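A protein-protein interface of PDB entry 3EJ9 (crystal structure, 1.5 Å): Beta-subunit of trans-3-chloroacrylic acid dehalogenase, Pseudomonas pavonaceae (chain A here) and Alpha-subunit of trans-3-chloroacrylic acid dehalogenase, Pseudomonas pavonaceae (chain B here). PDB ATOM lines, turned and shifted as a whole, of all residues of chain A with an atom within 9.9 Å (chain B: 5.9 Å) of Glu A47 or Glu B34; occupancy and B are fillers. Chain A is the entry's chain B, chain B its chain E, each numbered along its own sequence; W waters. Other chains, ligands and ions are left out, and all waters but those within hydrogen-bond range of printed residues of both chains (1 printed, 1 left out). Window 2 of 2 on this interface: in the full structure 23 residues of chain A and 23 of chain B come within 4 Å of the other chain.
The guanidinium group (NH1) of Arg A55 is in hydrogen-bond range of the side-chain amide oxygen (OD1) of Asn B38, at 3.1 Å.
O of Ile B28 sits at hydrogen-bond distance from OG1 of Thr B32 (2.7 Å).
The backbone carbonyl oxygen (O) of Glu B34 lies within hydrogen-bond range of the side-chain hydroxyl (OG) of Ser B29 (2.7 Å).
N of Glu B34 sits close to OG1 of Thr B32 (3.2 Å).
OE1 of Glu B34 lies within hydrogen-bond range of ND2 of Asn B38.
OG of Ser A51 sits at hydrogen-bond distance from O of Arg A55 (2.7 Å).
Among the printed residues, pairs that only touch across the chains: His A6 with Pro B2, Ile A52 with Asn B38, Ile A52 with Pro B2, Leu A19 with Ile B28 and Glu A47 with Glu B34.
Of chain B, only Glu B34 (3.8 Å) comes within 4 Å of Glu A47.
No residue of chain A comes within 4 Å of Ser B29.
Gly B33 touches none of the printed residues of chain A.
No residue of chain A comes within 4 Å of Pro B35.
Of the printed residues of chain B, Leu A19 touches Ile B28 (3.8 Å).
Printed residues of chain B within 4 Å of Arg A55: Asn B38 (3.1 Å).
Printed residues of chain B within 4 Å of His A6: Pro B2.
Printed residues of chain A within 4 Å of Pro B2: His A6 (3.2 Å) and Ile A52 (3.4 Å).
Arg B36 touches none of the printed residues of chain A.
The nearest residue of chain A that does not touch Glu B34 is Ala A8 (4.6 Å).
The nearest printed residue of chain B that does not touch Ile A52 is Ile B39 (4.3 Å).
Of the 12 printed residues of chain B, 4 touch a printed residue of chain A.
Among the printed residues, 6 pairs touch across the chains.
Among the printed residues, no Asp or Glu carboxylate lies within 4 Å of a Lys or Arg side-chain nitrogen of the other chain.
Water W1 bridges N of Ala A8 (2.8 Å) and OE2 of Glu B34 (3.3 Å).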
ATOM      1  N   HIS A   6       8.420  11.919  -3.623  1.00  0.00           N
ATOM      2  CA  HIS A   6       7.498  12.558  -4.555  1.00  0.00           C
ATOM      3  C   HIS A   6       6.775  13.656  -3.805  1.00  0.00           C
ATOM      4  O   HIS A   6       6.011  13.389  -2.868  1.00  0.00           O
ATOM      5  CB  HIS A   6       6.511  11.528  -5.090  1.00  0.00           C
ATOM      6  CG  HIS A   6       7.152  10.470  -5.927  1.00  0.00           C
ATOM      7  ND1 HIS A   6       7.438   9.210  -5.448  1.00  0.00           N
ATOM      8  CD2 HIS A   6       7.586  10.497  -7.207  1.00  0.00           C
ATOM      9  CE1 HIS A   6       8.018   8.503  -6.403  1.00  0.00           C
ATOM     10  NE2 HIS A   6       8.111   9.259  -7.482  1.00  0.00           N
ATOM     11  N   ILE A   7       7.046  14.889  -4.219  1.00  0.00           N
ATOM     12  CA  ILE A   7       6.496  16.077  -3.576  1.00  0.00           C
ATOM     13  C   ILE A   7       5.833  16.999  -4.593  1.00  0.00           C
ATOM     14  O   ILE A   7       6.024  16.859  -5.808  1.00  0.00           O
ATOM     15  CB  ILE A   7       7.586  16.853  -2.798  1.00  0.00           C
ATOM     16  CG1 ILE A   7       8.672  17.371  -3.751  1.00  0.00           C
ATOM     17  CG2 ILE A   7       8.159  15.981  -1.704  1.00  0.00           C
ATOM     18  CD1 ILE A   7       9.582  18.438  -3.156  1.00  0.00           C
ATOM     19  N   ALA A   8       5.042  17.933  -4.081  1.00  0.00           N
ATOM     20  CA  ALA A   8       4.420  18.937  -4.932  1.00  0.00           C
ATOM     21  C   ALA A   8       5.464  19.935  -5.388  1.00  0.00           C
ATOM     22  O   ALA A   8       6.404  20.261  -4.643  1.00  0.00           O
ATOM     23  CB  ALA A   8       3.292  19.651  -4.191  1.00  0.00           C
ATOM     24  N   THR A   9       5.295  20.416  -6.616  1.00  0.00           N
ATOM     25  CA  THR A   9       6.141  21.483  -7.137  1.00  0.00           C
ATOM     26  C   THR A   9       5.987  22.748  -6.285  1.00  0.00           C
ATOM     27  O   THR A   9       4.975  22.934  -5.593  1.00  0.00           O
ATOM     28  CB  THR A   9       5.856  21.764  -8.640  1.00  0.00           C
ATOM     29  OG1 THR A   9       6.865  22.631  -9.169  1.00  0.00           O
ATOM     30  CG2 THR A   9       4.479  22.397  -8.847  1.00  0.00           C
ATOM     31  N   GLY A  10       7.002  23.607  -6.309  1.00  0.00           N
ATOM     32  CA  GLY A  10       6.923  24.892  -5.605  1.00  0.00           C
ATOM     33  C   GLY A  10       8.097  25.273  -4.724  1.00  0.00           C
ATOM     34  O   GLY A  10       8.222  26.432  -4.329  1.00  0.00           O
ATOM     35  N   LEU A  11       8.952  24.306  -4.401  1.00  0.00           N
ATOM     36  CA  LEU A  11      10.146  24.596  -3.607  1.00  0.00           C
ATOM     37  C   LEU A  11      11.255  25.167  -4.479  1.00  0.00           C
ATOM     38  O   LEU A  11      11.326  24.885  -5.680  1.00  0.00           O
ATOM     39  CB  LEU A  11      10.647  23.346  -2.872  1.00  0.00           C
ATOM     40  CG  LEU A  11      10.003  22.929  -1.543  1.00  0.00           C
ATOM     41  CD1 LEU A  11       8.500  22.735  -1.627  1.00  0.00           C
ATOM     42  CD2 LEU A  11      10.671  21.674  -1.005  1.00  0.00           C
ATOM     43  N   LEU A  19      16.592  19.810   1.685  1.00  0.00           N
ATOM     44  CA  LEU A  19      15.771  18.615   1.878  1.00  0.00           C
ATOM     45  C   LEU A  19      16.579  17.326   1.681  1.00  0.00           C
ATOM     46  O   LEU A  19      16.494  16.406   2.497  1.00  0.00           O
ATOM     47  CB  LEU A  19      14.523  18.659   0.980  1.00  0.00           C
ATOM     48  CG  LEU A  19      13.564  17.464   1.004  1.00  0.00           C
ATOM     49  CD1 LEU A  19      13.109  17.108   2.417  1.00  0.00           C
ATOM     50  CD2 LEU A  19      12.356  17.681   0.091  1.00  0.00           C
ATOM     51  N   VAL A  43      11.437  14.034  -6.740  1.00  0.00           N
ATOM     52  CA  VAL A  43      10.617  14.184  -7.936  1.00  0.00           C
ATOM     53  C   VAL A  43       9.443  15.088  -7.611  1.00  0.00           C
ATOM     54  O   VAL A  43       8.762  14.890  -6.602  1.00  0.00           O
ATOM     55  CB  VAL A  43      10.093  12.834  -8.475  1.00  0.00           C
ATOM     56  CG1 VAL A  43       9.522  13.010  -9.879  1.00  0.00           C
ATOM     57  CG2 VAL A  43      11.189  11.768  -8.485  1.00  0.00           C
ATOM     58  N   GLU A  44       9.223  16.088  -8.461  1.00  0.00           N
ATOM     59  CA  GLU A  44       8.163  17.059  -8.250  1.00  0.00           C
ATOM     60  C   GLU A  44       6.979  16.805  -9.169  1.00  0.00           C
ATOM     61  O   GLU A  44       7.142  16.448 -10.344  1.00  0.00           O
ATOM     62  CB  GLU A  44       8.718  18.463  -8.439  1.00  0.00           C
ATOM     63  CG  GLU A  44       9.910  18.709  -7.536  1.00  0.00           C
ATOM     64  CD  GLU A  44      10.671  19.951  -7.908  1.00  0.00           C
ATOM     65  OE1 GLU A  44      10.169  21.060  -7.634  1.00  0.00           O
ATOM     66  OE2 GLU A  44      11.780  19.811  -8.470  1.00  0.00           O
ATOM     67  N   HIS A  45       5.785  17.007  -8.622  1.00  0.00           N
ATOM     68  CA  HIS A  45       4.550  16.734  -9.346  1.00  0.00           C
ATOM     69  C   HIS A  45       3.528  17.834  -9.130  1.00  0.00           C
ATOM     70  O   HIS A  45       3.533  18.509  -8.101  1.00  0.00           O
ATOM     71  CB  HIS A  45       3.936  15.410  -8.882  1.00  0.00           C
ATOM     72  CG  HIS A  45       4.877  14.250  -8.928  1.00  0.00           C
ATOM     73  ND1 HIS A  45       5.065  13.489 -10.061  1.00  0.00           N
ATOM     74  CD2 HIS A  45       5.673  13.713  -7.976  1.00  0.00           C
ATOM     75  CE1 HIS A  45       5.939  12.533  -9.806  1.00  0.00           C
ATOM     76  NE2 HIS A  45       6.327  12.650  -8.547  1.00  0.00           N
ATOM     77  N   ALA A  46       2.634  17.998 -10.098  1.00  0.00           N
ATOM     78  CA  ALA A  46       1.465  18.849  -9.913  1.00  0.00           C
ATOM     79  C   ALA A  46       0.564  18.205  -8.859  1.00  0.00           C
ATOM     80  O   ALA A  46       0.430  16.983  -8.810  1.00  0.00           O
ATOM     81  CB  ALA A  46       0.722  19.001 -11.221  1.00  0.00           C
ATOM     82  N   GLU A  47      -0.054  19.032  -8.021  1.00  0.00           N
ATOM     83  CA  GLU A  47      -0.939  18.545  -6.957  1.00  0.00           C
ATOM     84  C   GLU A  47      -2.071  17.653  -7.484  1.00  0.00           C
ATOM     85  O   GLU A  47      -2.450  16.670  -6.841  1.00  0.00           O
ATOM     86  CB  GLU A  47      -1.515  19.729  -6.164  1.00  0.00           C
ATOM     87  CG  GLU A  47      -0.480  20.490  -5.330  1.00  0.00           C
ATOM     88  CD  GLU A  47      -0.302  19.944  -3.918  1.00  0.00           C
ATOM     89  OE1 GLU A  47       0.102  20.728  -3.031  1.00  0.00           O
ATOM     90  OE2 GLU A  47      -0.557  18.743  -3.686  1.00  0.00           O
ATOM     91  N   ALA A  48      -2.590  18.003  -8.661  1.00  0.00           N
ATOM     92  CA  ALA A  48      -3.673  17.266  -9.315  1.00  0.00           C
ATOM     93  C   ALA A  48      -3.294  15.827  -9.657  1.00  0.00           C
ATOM     94  O   ALA A  48      -4.169  14.972  -9.803  1.00  0.00           O
ATOM     95  CB  ALA A  48      -4.109  17.996 -10.567  1.00  0.00           C
ATOM     96  N   ASN A  49      -1.995  15.565  -9.784  1.00  0.00           N
ATOM     97  CA  ASN A  49      -1.511  14.239 -10.174  1.00  0.00           C
ATOM     98  C   ASN A  49      -1.201  13.328  -8.986  1.00  0.00           C
ATOM     99  O   ASN A  49      -0.681  12.226  -9.175  1.00  0.00           O
ATOM    100  CB  ASN A  49      -0.277  14.363 -11.081  1.00  0.00           C
ATOM    101  CG  ASN A  49      -0.604  14.945 -12.461  1.00  0.00           C
ATOM    102  OD1 ASN A  49      -1.742  14.905 -12.921  1.00  0.00           O
ATOM    103  ND2 ASN A  49       0.411  15.484 -13.121  1.00  0.00           N
ATOM    104  N   MET A  50      -1.525  13.794  -7.780  1.00  0.00           N
ATOM    105  CA  MET A  50      -1.258  13.043  -6.551  1.00  0.00           C
ATOM    106  C   MET A  50      -2.519  12.891  -5.722  1.00  0.00           C
ATOM    107  O   MET A  50      -3.256  13.858  -5.519  1.00  0.00           O
ATOM    108  CB  MET A  50      -0.196  13.747  -5.703  1.00  0.00           C
ATOM    109  CG  MET A  50       1.170  13.873  -6.372  1.00  0.00           C
ATOM    110  SD  MET A  50       2.415  14.547  -5.263  1.00  0.00           S
ATOM    111  CE  MET A  50       1.923  16.262  -5.247  1.00  0.00           C
ATOM    112  N   SER A  51      -2.747  11.681  -5.222  1.00  0.00           N
ATOM    113  CA  SER A  51      -3.861  11.416  -4.316  1.00  0.00           C
ATOM    114  C   SER A  51      -3.396  10.587  -3.125  1.00  0.00           C
ATOM    115  O   SER A  51      -2.901   9.473  -3.284  1.00  0.00           O
ATOM    116  CB  SER A  51      -4.986  10.688  -5.052  1.00  0.00           C
ATOM    117  OG  SER A  51      -5.990  10.271  -4.141  1.00  0.00           O
ATOM    118  N   ILE A  52      -3.563  11.143  -1.932  1.00  0.00           N
ATOM    119  CA  ILE A  52      -3.242  10.458  -0.682  1.00  0.00           C
ATOM    120  C   ILE A  52      -4.544  10.130   0.008  1.00  0.00           C
ATOM    121  O   ILE A  52      -5.421  10.998   0.117  1.00  0.00           O
ATOM    122  CB  ILE A  52      -2.405  11.358   0.263  1.00  0.00           C
ATOM    123  CG1 ILE A  52      -1.121  11.835  -0.419  1.00  0.00           C
ATOM    124  CG2 ILE A  52      -2.084  10.648   1.585  1.00  0.00           C
ATOM    125  CD1 ILE A  52      -0.024  10.785  -0.548  1.00  0.00           C
ATOM    126  N   ARG A  55      -8.068  10.946  -1.572  1.00  0.00           N
ATOM    127  CA  ARG A  55      -8.523  12.328  -1.705  1.00  0.00           C
ATOM    128  C   ARG A  55      -8.207  12.892  -3.084  1.00  0.00           C
ATOM    129  O   ARG A  55      -7.122  12.668  -3.627  1.00  0.00           O
ATOM    130  CB  ARG A  55      -7.908  13.212  -0.616  1.00  0.00           C
ATOM    131  CG  ARG A  55      -8.433  12.926   0.787  1.00  0.00           C
ATOM    132  CD  ARG A  55      -7.918  13.937   1.802  1.00  0.00           C
ATOM    133  NE  ARG A  55      -6.480  13.797   2.035  1.00  0.00           N
ATOM    134  CZ  ARG A  55      -5.933  13.085   3.018  1.00  0.00           C
ATOM    135  NH1 ARG A  55      -4.615  13.031   3.132  1.00  0.00           N
ATOM    136  NH2 ARG A  55      -6.694  12.430   3.886  1.00  0.00           N
ATOM    137  N   ILE A  56      -9.164  13.627  -3.644  1.00  0.00           N
ATOM    138  CA  ILE A  56      -9.008  14.238  -4.960  1.00  0.00           C
ATOM    139  C   ILE A  56      -8.744  15.731  -4.783  1.00  0.00           C
ATOM    140  O   ILE A  56      -9.554  16.444  -4.179  1.00  0.00           O
ATOM    141  CB  ILE A  56     -10.267  14.022  -5.843  1.00  0.00           C
ATOM    142  CG1 ILE A  56     -10.598  12.525  -5.992  1.00  0.00           C
ATOM    143  CG2 ILE A  56     -10.121  14.734  -7.197  1.00  0.00           C
ATOM    144  CD1 ILE A  56      -9.534  11.680  -6.686  1.00  0.00           C
ATOM    145  N   HIS A  57      -7.603  16.192  -5.297  1.00  0.00           N
ATOM    146  CA  HIS A  57      -7.200  17.597  -5.172  1.00  0.00           C
ATOM    147  C   HIS A  57      -8.268  18.535  -5.733  1.00  0.00           C
ATOM    148  O   HIS A  57      -8.834  18.281  -6.797  1.00  0.00           O
ATOM    149  CB  HIS A  57      -5.849  17.842  -5.856  1.00  0.00           C
ATOM    150  CG  HIS A  57      -5.380  19.264  -5.779  1.00  0.00           C
ATOM    151  ND1 HIS A  57      -4.852  19.814  -4.631  1.00  0.00           N
ATOM    152  CD2 HIS A  57      -5.364  20.249  -6.710  1.00  0.00           C
ATOM    153  CE1 HIS A  57      -4.531  21.076  -4.856  1.00  0.00           C
ATOM    154  NE2 HIS A  57      -4.829  21.364  -6.110  1.00  0.00           N
ATOM    155  N   GLY A  58      -8.534  19.614  -5.001  1.00  0.00           N
ATOM    156  CA  GLY A  58      -9.591  20.558  -5.357  1.00  0.00           C
ATOM    157  C   GLY A  58     -10.835  20.363  -4.511  1.00  0.00           C
ATOM    158  O   GLY A  58     -11.543  21.326  -4.203  1.00  0.00           O
ATOM    159  N   GLU A  59     -11.100  19.111  -4.142  1.00  0.00           N
ATOM    160  CA  GLU A  59     -12.255  18.759  -3.319  1.00  0.00           C
ATOM    161  C   GLU A  59     -11.901  18.823  -1.837  1.00  0.00           C
ATOM    162  O   GLU A  59     -11.696  19.906  -1.286  1.00  0.00           O
ATOM    163  CB  GLU A  59     -12.769  17.361  -3.680  1.00  0.00           C
ATOM    164  CG  GLU A  59     -13.276  17.231  -5.117  1.00  0.00           C
ATOM    165  CD  GLU A  59     -14.028  15.934  -5.378  1.00  0.00           C
ATOM    166  OE1 GLU A  59     -14.734  15.863  -6.405  1.00  0.00           O
ATOM    167  OE2 GLU A  59     -13.924  14.990  -4.566  1.00  0.00           O
ATOM    168  N   PRO B   2       2.540  13.925  -0.123  1.00  0.00           N
ATOM    169  CA  PRO B   2       3.800  13.383  -0.597  1.00  0.00           C
ATOM    170  C   PRO B   2       3.842  11.882  -0.456  1.00  0.00           C
ATOM    171  O   PRO B   2       3.196  11.322   0.428  1.00  0.00           O
ATOM    172  CB  PRO B   2       4.820  14.018   0.354  1.00  0.00           C
ATOM    173  CG  PRO B   2       4.235  15.347   0.657  1.00  0.00           C
ATOM    174  CD  PRO B   2       2.732  15.223   0.554  1.00  0.00           C
ATOM    175  N   LEU B  25       9.174  11.537   7.707  1.00  0.00           N
ATOM    176  CA  LEU B  25       7.932  12.301   7.769  1.00  0.00           C
ATOM    177  C   LEU B  25       8.156  13.714   8.297  1.00  0.00           C
ATOM    178  O   LEU B  25       7.641  14.671   7.735  1.00  0.00           O
ATOM    179  CB  LEU B  25       6.879  11.566   8.598  1.00  0.00           C
ATOM    180  CG  LEU B  25       5.878  10.689   7.838  1.00  0.00           C
ATOM    181  CD1 LEU B  25       6.544   9.661   6.922  1.00  0.00           C
ATOM    182  CD2 LEU B  25       4.998   9.987   8.831  1.00  0.00           C
ATOM    183  N   ILE B  28      10.111  15.855   5.628  1.00  0.00           N
ATOM    184  CA  ILE B  28       9.227  16.170   4.511  1.00  0.00           C
ATOM    185  C   ILE B  28       8.172  17.195   4.916  1.00  0.00           C
ATOM    186  O   ILE B  28       7.927  18.149   4.174  1.00  0.00           O
ATOM    187  CB  ILE B  28       8.564  14.897   3.931  1.00  0.00           C
ATOM    188  CG1 ILE B  28       9.611  14.019   3.225  1.00  0.00           C
ATOM    189  CG2 ILE B  28       7.410  15.259   2.976  1.00  0.00           C
ATOM    190  CD1 ILE B  28      10.291  14.651   2.021  1.00  0.00           C
ATOM    191  N   SER B  29       7.568  17.011   6.091  1.00  0.00           N
ATOM    192  CA  SER B  29       6.577  17.959   6.593  1.00  0.00           C
ATOM    193  C   SER B  29       7.140  19.365   6.746  1.00  0.00           C
ATOM    194  O   SER B  29       6.495  20.330   6.340  1.00  0.00           O
ATOM    195  CB  SER B  29       5.973  17.492   7.925  1.00  0.00           C
ATOM    196  OG  SER B  29       4.929  18.365   8.322  1.00  0.00           O
ATOM    197  N   GLU B  30       8.338  19.481   7.320  1.00  0.00           N
ATOM    198  CA  GLU B  30       8.975  20.787   7.534  1.00  0.00           C
ATOM    199  C   GLU B  30       9.291  21.482   6.211  1.00  0.00           C
ATOM    200  O   GLU B  30       9.171  22.705   6.093  1.00  0.00           O
ATOM    201  CB  GLU B  30      10.271  20.628   8.324  1.00  0.00           C
ATOM    202  CG  GLU B  30      10.118  20.176   9.764  1.00  0.00           C
ATOM    203  CD  GLU B  30      11.460  19.879  10.418  1.00  0.00           C
ATOM    204  OE1 GLU B  30      11.482  19.543  11.619  1.00  0.00           O
ATOM    205  OE2 GLU B  30      12.500  19.977   9.727  1.00  0.00           O
ATOM    206  N   THR B  32       7.826  20.893   3.158  1.00  0.00           N
ATOM    207  CA  THR B  32       6.700  21.036   2.234  1.00  0.00           C
ATOM    208  C   THR B  32       5.462  21.679   2.849  1.00  0.00           C
ATOM    209  O   THR B  32       4.560  22.097   2.122  1.00  0.00           O
ATOM    210  CB  THR B  32       6.263  19.680   1.674  1.00  0.00           C
ATOM    211  OG1 THR B  32       5.778  18.865   2.745  1.00  0.00           O
ATOM    212  CG2 THR B  32       7.416  18.978   0.959  1.00  0.00           C
ATOM    213  N   GLY B  33       5.412  21.733   4.180  1.00  0.00           N
ATOM    214  CA  GLY B  33       4.242  22.233   4.898  1.00  0.00           C
ATOM    215  C   GLY B  33       3.079  21.256   4.899  1.00  0.00           C
ATOM    216  O   GLY B  33       1.963  21.600   5.304  1.00  0.00           O
ATOM    217  N   GLU B  34       3.343  20.032   4.455  1.00  0.00           N
ATOM    218  CA  GLU B  34       2.317  19.008   4.349  1.00  0.00           C
ATOM    219  C   GLU B  34       2.136  18.332   5.692  1.00  0.00           C
ATOM    220  O   GLU B  34       3.122  17.994   6.356  1.00  0.00           O
ATOM    221  CB  GLU B  34       2.697  17.977   3.286  1.00  0.00           C
ATOM    222  CG  GLU B  34       2.783  18.557   1.885  1.00  0.00           C
ATOM    223  CD  GLU B  34       1.479  18.501   1.131  1.00  0.00           C
ATOM    224  OE1 GLU B  34       0.433  18.194   1.746  1.00  0.00           O
ATOM    225  OE2 GLU B  34       1.504  18.769  -0.090  1.00  0.00           O
ATOM    226  N   PRO B  35       0.874  18.137   6.112  1.00  0.00           N
ATOM    227  CA  PRO B  35       0.622  17.474   7.380  1.00  0.00           C
ATOM    228  C   PRO B  35       0.942  15.980   7.340  1.00  0.00           C
ATOM    229  O   PRO B  35       0.979  15.361   6.271  1.00  0.00           O
ATOM    230  CB  PRO B  35      -0.881  17.681   7.590  1.00  0.00           C
ATOM    231  CG  PRO B  35      -1.433  17.818   6.217  1.00  0.00           C
ATOM    232  CD  PRO B  35      -0.376  18.532   5.435  1.00  0.00           C
ATOM    233  N   ARG B  36       1.176  15.430   8.523  1.00  0.00           N
ATOM    234  CA  ARG B  36       1.321  14.005   8.751  1.00  0.00           C
ATOM    235  C   ARG B  36       0.276  13.186   7.971  1.00  0.00           C
ATOM    236  O   ARG B  36       0.599  12.157   7.369  1.00  0.00           O
ATOM    237  CB  ARG B  36       1.198  13.769  10.261  1.00  0.00           C
ATOM    238  CG  ARG B  36       1.263  12.332  10.739  1.00  0.00           C
ATOM    239  CD  ARG B  36       1.050  12.310  12.255  1.00  0.00           C
ATOM    240  NE  ARG B  36       1.109  10.973  12.839  1.00  0.00           N
ATOM    241  CZ  ARG B  36       2.229  10.370  13.228  1.00  0.00           C
ATOM    242  NH1 ARG B  36       3.403  10.971  13.081  1.00  0.00           N
ATOM    243  NH2 ARG B  36       2.177   9.156  13.752  1.00  0.00           N
ATOM    244  N   ASN B  38      -1.131  13.764   5.186  1.00  0.00           N
ATOM    245  CA  ASN B  38      -0.986  13.780   3.734  1.00  0.00           C
ATOM    246  C   ASN B  38       0.313  13.156   3.235  1.00  0.00           C
ATOM    247  O   ASN B  38       0.716  13.404   2.105  1.00  0.00           O
ATOM    248  CB  ASN B  38      -1.117  15.203   3.180  1.00  0.00           C
ATOM    249  CG  ASN B  38      -1.599  15.226   1.732  1.00  0.00           C
ATOM    250  OD1 ASN B  38      -2.534  14.511   1.360  1.00  0.00           O
ATOM    251  ND2 ASN B  38      -0.972  16.062   0.911  1.00  0.00           N
ATOM    252  N   ILE B  39       0.960  12.343   4.066  1.00  0.00           N
ATOM    253  CA  ILE B  39       2.222  11.709   3.687  1.00  0.00           C
ATOM    254  C   ILE B  39       2.072  10.191   3.720  1.00  0.00           C
ATOM    255  O   ILE B  39       1.499   9.642   4.658  1.00  0.00           O
ATOM    256  CB  ILE B  39       3.396  12.183   4.606  1.00  0.00           C
ATOM    257  CG1 ILE B  39       3.568  13.704   4.534  1.00  0.00           C
ATOM    258  CG2 ILE B  39       4.711  11.495   4.246  1.00  0.00           C
ATOM    259  CD1 ILE B  39       4.456  14.288   5.630  1.00  0.00           C
HETATM  260  O   HOH W   1       4.498  18.256  -1.338  1.00  0.00           O
